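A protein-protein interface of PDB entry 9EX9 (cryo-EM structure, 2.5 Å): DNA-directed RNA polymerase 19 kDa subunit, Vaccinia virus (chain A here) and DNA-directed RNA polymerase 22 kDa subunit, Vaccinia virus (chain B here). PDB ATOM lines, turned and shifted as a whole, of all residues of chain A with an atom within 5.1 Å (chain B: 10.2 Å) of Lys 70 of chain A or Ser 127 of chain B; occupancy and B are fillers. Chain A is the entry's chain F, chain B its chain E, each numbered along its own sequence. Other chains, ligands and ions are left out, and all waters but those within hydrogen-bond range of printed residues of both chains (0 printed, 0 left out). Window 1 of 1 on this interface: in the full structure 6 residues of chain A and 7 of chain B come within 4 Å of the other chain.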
ATOM      1  N   GLY A  63     -21.345 -14.193  -5.469  1.00  0.00           N
ATOM      2  CA  GLY A  63     -22.460 -13.298  -5.223  1.00  0.00           C
ATOM      3  C   GLY A  63     -22.680 -12.313  -6.351  1.00  0.00           C
ATOM      4  O   GLY A  63     -23.817 -11.922  -6.627  1.00  0.00           O
ATOM      5  N   HIS A  65     -22.229 -12.933  -9.527  1.00  0.00           N
ATOM      6  CA  HIS A  65     -22.919 -13.642 -10.597  1.00  0.00           C
ATOM      7  C   HIS A  65     -24.420 -13.684 -10.343  1.00  0.00           C
ATOM      8  O   HIS A  65     -25.227 -13.402 -11.239  1.00  0.00           O
ATOM      9  CB  HIS A  65     -22.348 -15.052 -10.718  1.00  0.00           C
ATOM     10  CG  HIS A  65     -22.709 -15.745 -11.992  1.00  0.00           C
ATOM     11  ND1 HIS A  65     -22.630 -15.129 -13.221  1.00  0.00           N
ATOM     12  CD2 HIS A  65     -23.139 -17.006 -12.229  1.00  0.00           C
ATOM     13  CE1 HIS A  65     -23.003 -15.978 -14.161  1.00  0.00           C
ATOM     14  NE2 HIS A  65     -23.315 -17.125 -13.586  1.00  0.00           N
ATOM     15  N   ILE A  66     -24.813 -14.024  -9.117  1.00  0.00           N
ATOM     16  CA  ILE A  66     -26.232 -14.091  -8.788  1.00  0.00           C
ATOM     17  C   ILE A  66     -26.853 -12.704  -8.838  1.00  0.00           C
ATOM     18  O   ILE A  66     -27.999 -12.536  -9.269  1.00  0.00           O
ATOM     19  CB  ILE A  66     -26.428 -14.752  -7.413  1.00  0.00           C
ATOM     20  CG1 ILE A  66     -25.808 -16.151  -7.388  1.00  0.00           C
ATOM     21  CG2 ILE A  66     -27.900 -14.822  -7.067  1.00  0.00           C
ATOM     22  CD1 ILE A  66     -26.435 -17.129  -8.356  1.00  0.00           C
ATOM     23  N   SER A  67     -26.112 -11.685  -8.400  1.00  0.00           N
ATOM     24  CA  SER A  67     -26.624 -10.324  -8.474  1.00  0.00           C
ATOM     25  C   SER A  67     -26.893  -9.919  -9.916  1.00  0.00           C
ATOM     26  O   SER A  67     -27.924  -9.307 -10.214  1.00  0.00           O
ATOM     27  CB  SER A  67     -25.636  -9.361  -7.827  1.00  0.00           C
ATOM     28  OG  SER A  67     -25.323  -9.773  -6.510  1.00  0.00           O
ATOM     29  N   ALA A  68     -25.972 -10.249 -10.824  1.00  0.00           N
ATOM     30  CA  ALA A  68     -26.170  -9.926 -12.232  1.00  0.00           C
ATOM     31  C   ALA A  68     -27.364 -10.672 -12.808  1.00  0.00           C
ATOM     32  O   ALA A  68     -28.171 -10.096 -13.551  1.00  0.00           O
ATOM     33  CB  ALA A  68     -24.907 -10.254 -13.021  1.00  0.00           C
ATOM     34  N   LEU A  69     -27.497 -11.957 -12.479  1.00  0.00           N
ATOM     35  CA  LEU A  69     -28.644 -12.711 -12.973  1.00  0.00           C
ATOM     36  C   LEU A  69     -29.947 -12.095 -12.488  1.00  0.00           C
ATOM     37  O   LEU A  69     -30.907 -11.974 -13.254  1.00  0.00           O
ATOM     38  CB  LEU A  69     -28.551 -14.171 -12.533  1.00  0.00           C
ATOM     39  CG  LEU A  69     -27.491 -15.040 -13.208  1.00  0.00           C
ATOM     40  CD1 LEU A  69     -27.450 -16.402 -12.557  1.00  0.00           C
ATOM     41  CD2 LEU A  69     -27.764 -15.176 -14.689  1.00  0.00           C
ATOM     42  N   LYS A  70     -29.999 -11.691 -11.222  1.00  0.00           N
ATOM     43  CA  LYS A  70     -31.216 -11.095 -10.685  1.00  0.00           C
ATOM     44  C   LYS A  70     -31.500  -9.733 -11.314  1.00  0.00           C
ATOM     45  O   LYS A  70     -32.659  -9.391 -11.580  1.00  0.00           O
ATOM     46  CB  LYS A  70     -31.100 -10.994  -9.167  1.00  0.00           C
ATOM     47  CG  LYS A  70     -31.030 -12.351  -8.477  1.00  0.00           C
ATOM     48  CD  LYS A  70     -30.714 -12.238  -6.997  1.00  0.00           C
ATOM     49  CE  LYS A  70     -31.879 -11.679  -6.210  1.00  0.00           C
ATOM     50  NZ  LYS A  70     -31.533 -11.459  -4.784  1.00  0.00           N
ATOM     51  N   ARG A  71     -30.456  -8.938 -11.562  1.00  0.00           N
ATOM     52  CA  ARG A  71     -30.655  -7.660 -12.236  1.00  0.00           C
ATOM     53  C   ARG A  71     -31.246  -7.860 -13.622  1.00  0.00           C
ATOM     54  O   ARG A  71     -32.151  -7.126 -14.029  1.00  0.00           O
ATOM     55  CB  ARG A  71     -29.338  -6.897 -12.334  1.00  0.00           C
ATOM     56  CG  ARG A  71     -29.033  -6.041 -11.135  1.00  0.00           C
ATOM     57  CD  ARG A  71     -27.985  -5.002 -11.464  1.00  0.00           C
ATOM     58  NE  ARG A  71     -26.728  -5.600 -11.896  1.00  0.00           N
ATOM     59  CZ  ARG A  71     -25.747  -5.959 -11.080  1.00  0.00           C
ATOM     60  NH1 ARG A  71     -25.846  -5.812  -9.769  1.00  0.00           N
ATOM     61  NH2 ARG A  71     -24.636  -6.479 -11.593  1.00  0.00           N
ATOM     62  N   ARG A  72     -30.742  -8.844 -14.368  1.00  0.00           N
ATOM     63  CA  ARG A  72     -31.350  -9.151 -15.658  1.00  0.00           C
ATOM     64  C   ARG A  72     -32.789  -9.617 -15.483  1.00  0.00           C
ATOM     65  O   ARG A  72     -33.675  -9.223 -16.248  1.00  0.00           O
ATOM     66  CB  ARG A  72     -30.533 -10.204 -16.395  1.00  0.00           C
ATOM     67  CG  ARG A  72     -29.244  -9.671 -16.978  1.00  0.00           C
ATOM     68  CD  ARG A  72     -28.546 -10.708 -17.837  1.00  0.00           C
ATOM     69  NE  ARG A  72     -29.323 -11.056 -19.022  1.00  0.00           N
ATOM     70  CZ  ARG A  72     -29.295 -10.384 -20.164  1.00  0.00           C
ATOM     71  NH1 ARG A  72     -28.543  -9.306 -20.316  1.00  0.00           N
ATOM     72  NH2 ARG A  72     -30.043 -10.800 -21.180  1.00  0.00           N
ATOM     73  N   TYR A  73     -33.040 -10.456 -14.478  1.00  0.00           N
ATOM     74  CA  TYR A  73     -34.396 -10.924 -14.222  1.00  0.00           C
ATOM     75  C   TYR A  73     -35.345  -9.762 -13.970  1.00  0.00           C
ATOM     76  O   TYR A  73     -36.538  -9.860 -14.263  1.00  0.00           O
ATOM     77  CB  TYR A  73     -34.395 -11.878 -13.027  1.00  0.00           C
ATOM     78  CG  TYR A  73     -35.644 -12.710 -12.904  1.00  0.00           C
ATOM     79  CD1 TYR A  73     -35.757 -13.922 -13.556  1.00  0.00           C
ATOM     80  CD2 TYR A  73     -36.711 -12.282 -12.140  1.00  0.00           C
ATOM     81  CE1 TYR A  73     -36.896 -14.682 -13.454  1.00  0.00           C
ATOM     82  CE2 TYR A  73     -37.854 -13.036 -12.032  1.00  0.00           C
ATOM     83  CZ  TYR A  73     -37.941 -14.234 -12.690  1.00  0.00           C
ATOM     84  OH  TYR A  73     -39.080 -14.989 -12.584  1.00  0.00           O
ATOM     85  N   THR A  74     -34.833  -8.656 -13.434  1.00  0.00           N
ATOM     86  CA  THR A  74     -35.689  -7.520 -13.103  1.00  0.00           C
ATOM     87  C   THR A  74     -36.396  -6.927 -14.319  1.00  0.00           C
ATOM     88  O   THR A  74     -37.390  -6.215 -14.151  1.00  0.00           O
ATOM     89  CB  THR A  74     -34.859  -6.429 -12.422  1.00  0.00           C
ATOM     90  OG1 THR A  74     -34.395  -6.903 -11.156  1.00  0.00           O
ATOM     91  CG2 THR A  74     -35.676  -5.166 -12.218  1.00  0.00           C
ATOM     92  N   LEU B 117     -25.250 -27.644   3.605  1.00  0.00           N
ATOM     93  CA  LEU B 117     -24.680 -26.860   2.521  1.00  0.00           C
ATOM     94  C   LEU B 117     -23.223 -26.522   2.805  1.00  0.00           C
ATOM     95  O   LEU B 117     -22.832 -26.283   3.950  1.00  0.00           O
ATOM     96  CB  LEU B 117     -25.465 -25.565   2.326  1.00  0.00           C
ATOM     97  CG  LEU B 117     -26.967 -25.701   2.133  1.00  0.00           C
ATOM     98  CD1 LEU B 117     -27.583 -24.336   1.933  1.00  0.00           C
ATOM     99  CD2 LEU B 117     -27.257 -26.594   0.960  1.00  0.00           C
ATOM    100  N   THR B 119     -19.755 -23.989   1.746  1.00  0.00           N
ATOM    101  CA  THR B 119     -19.592 -22.538   1.777  1.00  0.00           C
ATOM    102  C   THR B 119     -20.111 -21.883   0.500  1.00  0.00           C
ATOM    103  O   THR B 119     -20.770 -20.837   0.555  1.00  0.00           O
ATOM    104  CB  THR B 119     -18.125 -22.181   2.010  1.00  0.00           C
ATOM    105  OG1 THR B 119     -17.986 -20.758   2.067  1.00  0.00           O
ATOM    106  CG2 THR B 119     -17.245 -22.726   0.897  1.00  0.00           C
ATOM    107  N   THR B 120     -19.824 -22.476  -0.659  1.00  0.00           N
ATOM    108  CA  THR B 120     -20.268 -21.890  -1.920  1.00  0.00           C
ATOM    109  C   THR B 120     -21.788 -21.857  -2.003  1.00  0.00           C
ATOM    110  O   THR B 120     -22.385 -20.839  -2.381  1.00  0.00           O
ATOM    111  CB  THR B 120     -19.686 -22.678  -3.090  1.00  0.00           C
ATOM    112  OG1 THR B 120     -18.256 -22.613  -3.048  1.00  0.00           O
ATOM    113  CG2 THR B 120     -20.174 -22.118  -4.406  1.00  0.00           C
ATOM    114  N   GLU B 121     -22.434 -22.966  -1.650  1.00  0.00           N
ATOM    115  CA  GLU B 121     -23.890 -23.006  -1.678  1.00  0.00           C
ATOM    116  C   GLU B 121     -24.474 -22.032  -0.669  1.00  0.00           C
ATOM    117  O   GLU B 121     -25.514 -21.412  -0.921  1.00  0.00           O
ATOM    118  CB  GLU B 121     -24.369 -24.427  -1.405  1.00  0.00           C
ATOM    119  CG  GLU B 121     -23.893 -25.426  -2.439  1.00  0.00           C
ATOM    120  CD  GLU B 121     -24.094 -26.861  -2.006  1.00  0.00           C
ATOM    121  OE1 GLU B 121     -24.101 -27.123  -0.787  1.00  0.00           O
ATOM    122  OE2 GLU B 121     -24.243 -27.733  -2.886  1.00  0.00           O
ATOM    123  N   THR B 122     -23.818 -21.880   0.480  1.00  0.00           N
ATOM    124  CA  THR B 122     -24.280 -20.914   1.467  1.00  0.00           C
ATOM    125  C   THR B 122     -24.233 -19.500   0.910  1.00  0.00           C
ATOM    126  O   THR B 122     -25.171 -18.718   1.100  1.00  0.00           O
ATOM    127  CB  THR B 122     -23.430 -21.014   2.730  1.00  0.00           C
ATOM    128  OG1 THR B 122     -23.527 -22.336   3.270  1.00  0.00           O
ATOM    129  CG2 THR B 122     -23.896 -20.011   3.765  1.00  0.00           C
ATOM    130  N   ASN B 123     -23.142 -19.153   0.221  1.00  0.00           N
ATOM    131  CA  ASN B 123     -23.052 -17.829  -0.386  1.00  0.00           C
ATOM    132  C   ASN B 123     -24.134 -17.635  -1.435  1.00  0.00           C
ATOM    133  O   ASN B 123     -24.734 -16.557  -1.528  1.00  0.00           O
ATOM    134  CB  ASN B 123     -21.673 -17.623  -1.005  1.00  0.00           C
ATOM    135  CG  ASN B 123     -20.596 -17.440   0.030  1.00  0.00           C
ATOM    136  OD1 ASN B 123     -20.881 -17.222   1.203  1.00  0.00           O
ATOM    137  ND2 ASN B 123     -19.345 -17.519  -0.397  1.00  0.00           N
ATOM    138  N   ILE B 124     -24.398 -18.664  -2.238  1.00  0.00           N
ATOM    139  CA  ILE B 124     -25.456 -18.552  -3.239  1.00  0.00           C
ATOM    140  C   ILE B 124     -26.799 -18.296  -2.569  1.00  0.00           C
ATOM    141  O   ILE B 124     -27.577 -17.447  -3.018  1.00  0.00           O
ATOM    142  CB  ILE B 124     -25.494 -19.809  -4.125  1.00  0.00           C
ATOM    143  CG1 ILE B 124     -24.273 -19.831  -5.042  1.00  0.00           C
ATOM    144  CG2 ILE B 124     -26.779 -19.841  -4.928  1.00  0.00           C
ATOM    145  CD1 ILE B 124     -24.105 -21.110  -5.811  1.00  0.00           C
ATOM    146  N   VAL B 125     -27.101 -19.024  -1.495  1.00  0.00           N
ATOM    147  CA  VAL B 125     -28.382 -18.836  -0.815  1.00  0.00           C
ATOM    148  C   VAL B 125     -28.476 -17.429  -0.239  1.00  0.00           C
ATOM    149  O   VAL B 125     -29.501 -16.747  -0.376  1.00  0.00           O
ATOM    150  CB  VAL B 125     -28.576 -19.902   0.277  1.00  0.00           C
ATOM    151  CG1 VAL B 125     -29.832 -19.616   1.065  1.00  0.00           C
ATOM    152  CG2 VAL B 125     -28.653 -21.281  -0.335  1.00  0.00           C
ATOM    153  N   ASN B 126     -27.408 -16.972   0.416  1.00  0.00           N
ATOM    154  CA  ASN B 126     -27.427 -15.637   1.003  1.00  0.00           C
ATOM    155  C   ASN B 126     -27.640 -14.577  -0.063  1.00  0.00           C
ATOM    156  O   ASN B 126     -28.407 -13.630   0.137  1.00  0.00           O
ATOM    157  CB  ASN B 126     -26.127 -15.370   1.756  1.00  0.00           C
ATOM    158  CG  ASN B 126     -26.090 -16.033   3.110  1.00  0.00           C
ATOM    159  OD1 ASN B 126     -27.126 -16.370   3.676  1.00  0.00           O
ATOM    160  ND2 ASN B 126     -24.891 -16.216   3.643  1.00  0.00           N
ATOM    161  N   SER B 127     -26.966 -14.717  -1.203  1.00  0.00           N
ATOM    162  CA  SER B 127     -27.141 -13.758  -2.285  1.00  0.00           C
ATOM    163  C   SER B 127     -28.561 -13.796  -2.827  1.00  0.00           C
ATOM    164  O   SER B 127     -29.148 -12.752  -3.124  1.00  0.00           O
ATOM    165  CB  SER B 127     -26.136 -14.042  -3.395  1.00  0.00           C
ATOM    166  OG  SER B 127     -26.251 -13.084  -4.423  1.00  0.00           O
ATOM    167  N   VAL B 128     -29.131 -14.992  -2.967  1.00  0.00           N
ATOM    168  CA  VAL B 128     -30.484 -15.100  -3.493  1.00  0.00           C
ATOM    169  C   VAL B 128     -31.495 -14.490  -2.537  1.00  0.00           C
ATOM    170  O   VAL B 128     -32.564 -14.042  -2.963  1.00  0.00           O
ATOM    171  CB  VAL B 128     -30.826 -16.568  -3.798  1.00  0.00           C
ATOM    172  CG1 VAL B 128     -32.308 -16.719  -4.060  1.00  0.00           C
ATOM    173  CG2 VAL B 128     -30.033 -17.055  -4.989  1.00  0.00           C
ATOM    174  N   LEU B 129     -31.198 -14.471  -1.237  1.00  0.00           N
ATOM    175  CA  LEU B 129     -32.183 -13.976  -0.281  1.00  0.00           C
ATOM    176  C   LEU B 129     -32.294 -12.457  -0.254  1.00  0.00           C
ATOM    177  O   LEU B 129     -33.320 -11.939   0.195  1.00  0.00           O
ATOM    178  CB  LEU B 129     -31.858 -14.487   1.122  1.00  0.00           C
ATOM    179  CG  LEU B 129     -32.253 -15.936   1.405  1.00  0.00           C
ATOM    180  CD1 LEU B 129     -31.758 -16.352   2.768  1.00  0.00           C
ATOM    181  CD2 LEU B 129     -33.754 -16.121   1.311  1.00  0.00           C
ATOM    182  N   GLN B 130     -31.278 -11.728  -0.710  1.00  0.00           N
ATOM    183  CA  GLN B 130     -31.338 -10.273  -0.675  1.00  0.00           C
ATOM    184  C   GLN B 130     -32.423  -9.751  -1.608  1.00  0.00           C
ATOM    185  O   GLN B 130     -32.705 -10.332  -2.658  1.00  0.00           O
ATOM    186  CB  GLN B 130     -29.994  -9.671  -1.063  1.00  0.00           C
ATOM    187  CG  GLN B 130     -28.922  -9.852  -0.024  1.00  0.00           C
ATOM    188  CD  GLN B 130     -27.579  -9.357  -0.496  1.00  0.00           C
ATOM    189  OE1 GLN B 130     -27.486  -8.627  -1.478  1.00  0.00           O
ATOM    190  NE2 GLN B 130     -26.524  -9.759   0.197  1.00  0.00           N
ATOM    191  N   THR B 131     -33.034  -8.636  -1.215  1.00  0.00           N
ATOM    192  CA  THR B 131     -34.126  -8.041  -1.974  1.00  0.00           C
ATOM    193  C   THR B 131     -33.657  -7.055  -3.033  1.00  0.00           C
ATOM    194  O   THR B 131     -34.484  -6.562  -3.804  1.00  0.00           O
ATOM    195  CB  THR B 131     -35.097  -7.325  -1.034  1.00  0.00           C
ATOM    196  OG1 THR B 131     -34.381  -6.370  -0.247  1.00  0.00           O
ATOM    197  CG2 THR B 131     -35.787  -8.315  -0.116  1.00  0.00           C
ATOM    198  N   GLY B 132     -32.365  -6.745  -3.086  1.00  0.00           N
ATOM    199  CA  GLY B 132     -31.844  -5.828  -4.072  1.00  0.00           C
ATOM    200  C   GLY B 132     -32.004  -4.366  -3.726  1.00  0.00           C
ATOM    201  O   GLY B 132     -31.530  -3.514  -4.487  1.00  0.00           O
ATOM    202  N   ASP B 133     -32.645  -4.047  -2.607  1.00  0.00           N
ATOM    203  CA  ASP B 133     -32.882  -2.672  -2.178  1.00  0.00           C
ATOM    204  C   ASP B 133     -32.005  -2.410  -0.958  1.00  0.00           C
ATOM    205  O   ASP B 133     -32.443  -2.552   0.184  1.00  0.00           O
ATOM    206  CB  ASP B 133     -34.359  -2.453  -1.870  1.00  0.00           C
ATOM    207  CG  ASP B 133     -34.637  -1.089  -1.279  1.00  0.00           C
ATOM    208  OD1 ASP B 133     -34.342  -0.077  -1.947  1.00  0.00           O
ATOM    209  OD2 ASP B 133     -35.160  -1.029  -0.147  1.00  0.00           O
ATOM    210  N   GLY B 134     -30.760  -2.016  -1.207  1.00  0.00           N
ATOM    211  CA  GLY B 134     -29.818  -1.793  -0.131  1.00  0.00           C
ATOM    212  C   GLY B 134     -29.270  -3.088   0.427  1.00  0.00           C
ATOM    213  O   GLY B 134     -28.612  -3.849  -0.288  1.00  0.00           O
ATOM    214  N   LYS B 135     -29.534  -3.350   1.707  1.00  0.00           N
ATOM    215  CA  LYS B 135     -29.104  -4.584   2.353  1.00  0.00           C
ATOM    216  C   LYS B 135     -30.265  -5.361   2.958  1.00  0.00           C
ATOM    217  O   LYS B 135     -30.032  -6.358   3.652  1.00  0.00           O
ATOM    218  CB  LYS B 135     -28.061  -4.283   3.432  1.00  0.00           C
ATOM    219  CG  LYS B 135     -26.713  -3.861   2.879  1.00  0.00           C
ATOM    220  CD  LYS B 135     -25.692  -3.675   3.989  1.00  0.00           C
ATOM    221  CE  LYS B 135     -24.325  -3.311   3.434  1.00  0.00           C
ATOM    222  NZ  LYS B 135     -23.323  -3.098   4.514  1.00  0.00           N
ATOM    223  N   LYS B 136     -31.503  -4.942   2.716  1.00  0.00           N
ATOM    224  CA  LYS B 136     -32.646  -5.686   3.222  1.00  0.00           C
ATOM    225  C   LYS B 136     -32.646  -7.096   2.645  1.00  0.00           C
ATOM    226  O   LYS B 136     -32.290  -7.314   1.485  1.00  0.00           O
ATOM    227  CB  LYS B 136     -33.946  -4.971   2.865  1.00  0.00           C
ATOM    228  CG  LYS B 136     -34.040  -3.568   3.418  1.00  0.00           C
ATOM    229  CD  LYS B 136     -35.367  -2.926   3.067  1.00  0.00           C
ATOM    230  CE  LYS B 136     -35.463  -1.518   3.626  1.00  0.00           C
ATOM    231  NZ  LYS B 136     -36.786  -0.899   3.348  1.00  0.00           N
ATOM    232  N   THR B 137     -33.046  -8.059   3.470  1.00  0.00           N
ATOM    233  CA  THR B 137     -32.971  -9.459   3.086  1.00  0.00           C
ATOM    234  C   THR B 137     -34.143 -10.217   3.686  1.00  0.00           C
ATOM    235  O   THR B 137     -34.734  -9.801   4.683  1.00  0.00           O
ATOM    236  CB  THR B 137     -31.649 -10.088   3.534  1.00  0.00           C
ATOM    237  OG1 THR B 137     -31.681 -11.496   3.293  1.00  0.00           O
ATOM    238  CG2 THR B 137     -31.411  -9.839   5.007  1.00  0.00           C
ATOM    239  N   LEU B 138     -34.475 -11.337   3.054  1.00  0.00           N
ATOM    240  CA  LEU B 138     -35.494 -12.240   3.559  1.00  0.00           C
ATOM    241  C   LEU B 138     -34.877 -13.241   4.530  1.00  0.00           C
ATOM    242  O   LEU B 138     -33.661 -13.303   4.715  1.00  0.00           O
ATOM    243  CB  LEU B 138     -36.178 -12.976   2.410  1.00  0.00           C
ATOM    244  CG  LEU B 138     -36.912 -12.127   1.376  1.00  0.00           C
ATOM    245  CD1 LEU B 138     -37.301 -12.981   0.190  1.00  0.00           C
ATOM    246  CD2 LEU B 138     -38.137 -11.482   1.978  1.00  0.00           C
ATOM    247  N   LEU B 140     -35.124 -17.415   6.033  1.00  0.00           N
ATOM    248  CA  LEU B 140     -35.617 -18.768   5.859  1.00  0.00           C
ATOM    249  C   LEU B 140     -36.452 -19.182   7.064  1.00  0.00           C
ATOM    250  O   LEU B 140     -36.224 -18.703   8.176  1.00  0.00           O
ATOM    251  CB  LEU B 140     -34.458 -19.738   5.689  1.00  0.00           C
ATOM    252  CG  LEU B 140     -33.615 -19.568   4.432  1.00  0.00           C
ATOM    253  CD1 LEU B 140     -32.393 -20.450   4.510  1.00  0.00           C
ATOM    254  CD2 LEU B 140     -34.430 -19.896   3.202  1.00  0.00           C
ATOM    255  N   ILE B 162     -27.672 -23.645   8.126  1.00  0.00           N
ATOM    256  CA  ILE B 162     -28.738 -23.909   7.170  1.00  0.00           C
ATOM    257  C   ILE B 162     -28.739 -25.393   6.840  1.00  0.00           C
ATOM    258  O   ILE B 162     -27.677 -26.005   6.685  1.00  0.00           O
ATOM    259  CB  ILE B 162     -28.580 -23.068   5.887  1.00  0.00           C
ATOM    260  CG1 ILE B 162     -28.520 -21.583   6.231  1.00  0.00           C
ATOM    261  CG2 ILE B 162     -29.735 -23.330   4.936  1.00  0.00           C
ATOM    262  CD1 ILE B 162     -28.255 -20.696   5.044  1.00  0.00           C
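The side-chain amino group (NZ) of Lys 70 of chain A lies within hydrogen-bond range of the backbone carbonyl oxygen (O) of Val 128 of chain B, 3.3 Å away. The backbone carbonyl oxygen (O) of Gln 130 of chain B lies within hydrogen-bond range of the side-chain amino group (NZ) of Lys 70 of chain A (2.7 Å). OG of Ser 127 of chain B sits at hydrogen-bond distance from O of Gly 63 of chain A (3.5 Å). O of Ser 127 of chain B sits at hydrogen-bond distance from NZ of Lys 70 of chain A (3.2 Å).
The side-chain hydroxyl of Thr 74 of chain A sits at hydrogen-bond distance from the backbone carbonyl oxygen of Lys 70 of chain A, 3.1 Å away. O of Gly 63 of chain A lies within hydrogen-bond range of OG of Ser 67 of chain A (2.6 Å).
OG of Ser 127 of chain B touches CB of Ile 66 of chain A, 3.4 Å away. Ile 66 of chain A touches Val 128 of chain B (CG2 to CG2, 3.7 Å).
Of the printed residues of chain B, Lys 70 of chain A touches Ser 127 (3.2 Å), Val 128 (3.3 Å) and Gln 130 (2.7 Å). Of the printed residues of chain A, Ser 127 of chain B touches Gly 63 (3.5 Å), Ile 66 (3.4 Å) and Lys 70 (3.2 Å). Of the printed residues of chain B, Gly 63 of chain A touches Ser 127 (3.5 Å). Ile 66 of chain A touches just these residues of chain B: Ser 127 and Val 128. No residue of chain B comes within 4 Å of Ser 67 of chain A. No residue of chain B comes within 4 Å of Ala 68 of chain A. Printed residues of chain A within 4 Å of Val 128 of chain B: Ile 66 and Lys 70. Printed residues of chain A within 4 Å of Gln 130 of chain B: Lys 70.
Of the 23 printed residues of chain B, 3 touch a printed residue of chain A. Hydrophobic or aromatic side chains of chain B within 4 Å of the printed part of chain A: Val 128. Hydrophobic or aromatic side chains of chain A within 4 Å of the printed part of chain B: Ile 66. Among the printed residues, no Asp or Glu carboxylate lies within 4 Å of a Lys or Arg side-chain nitrogen of the other chain.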
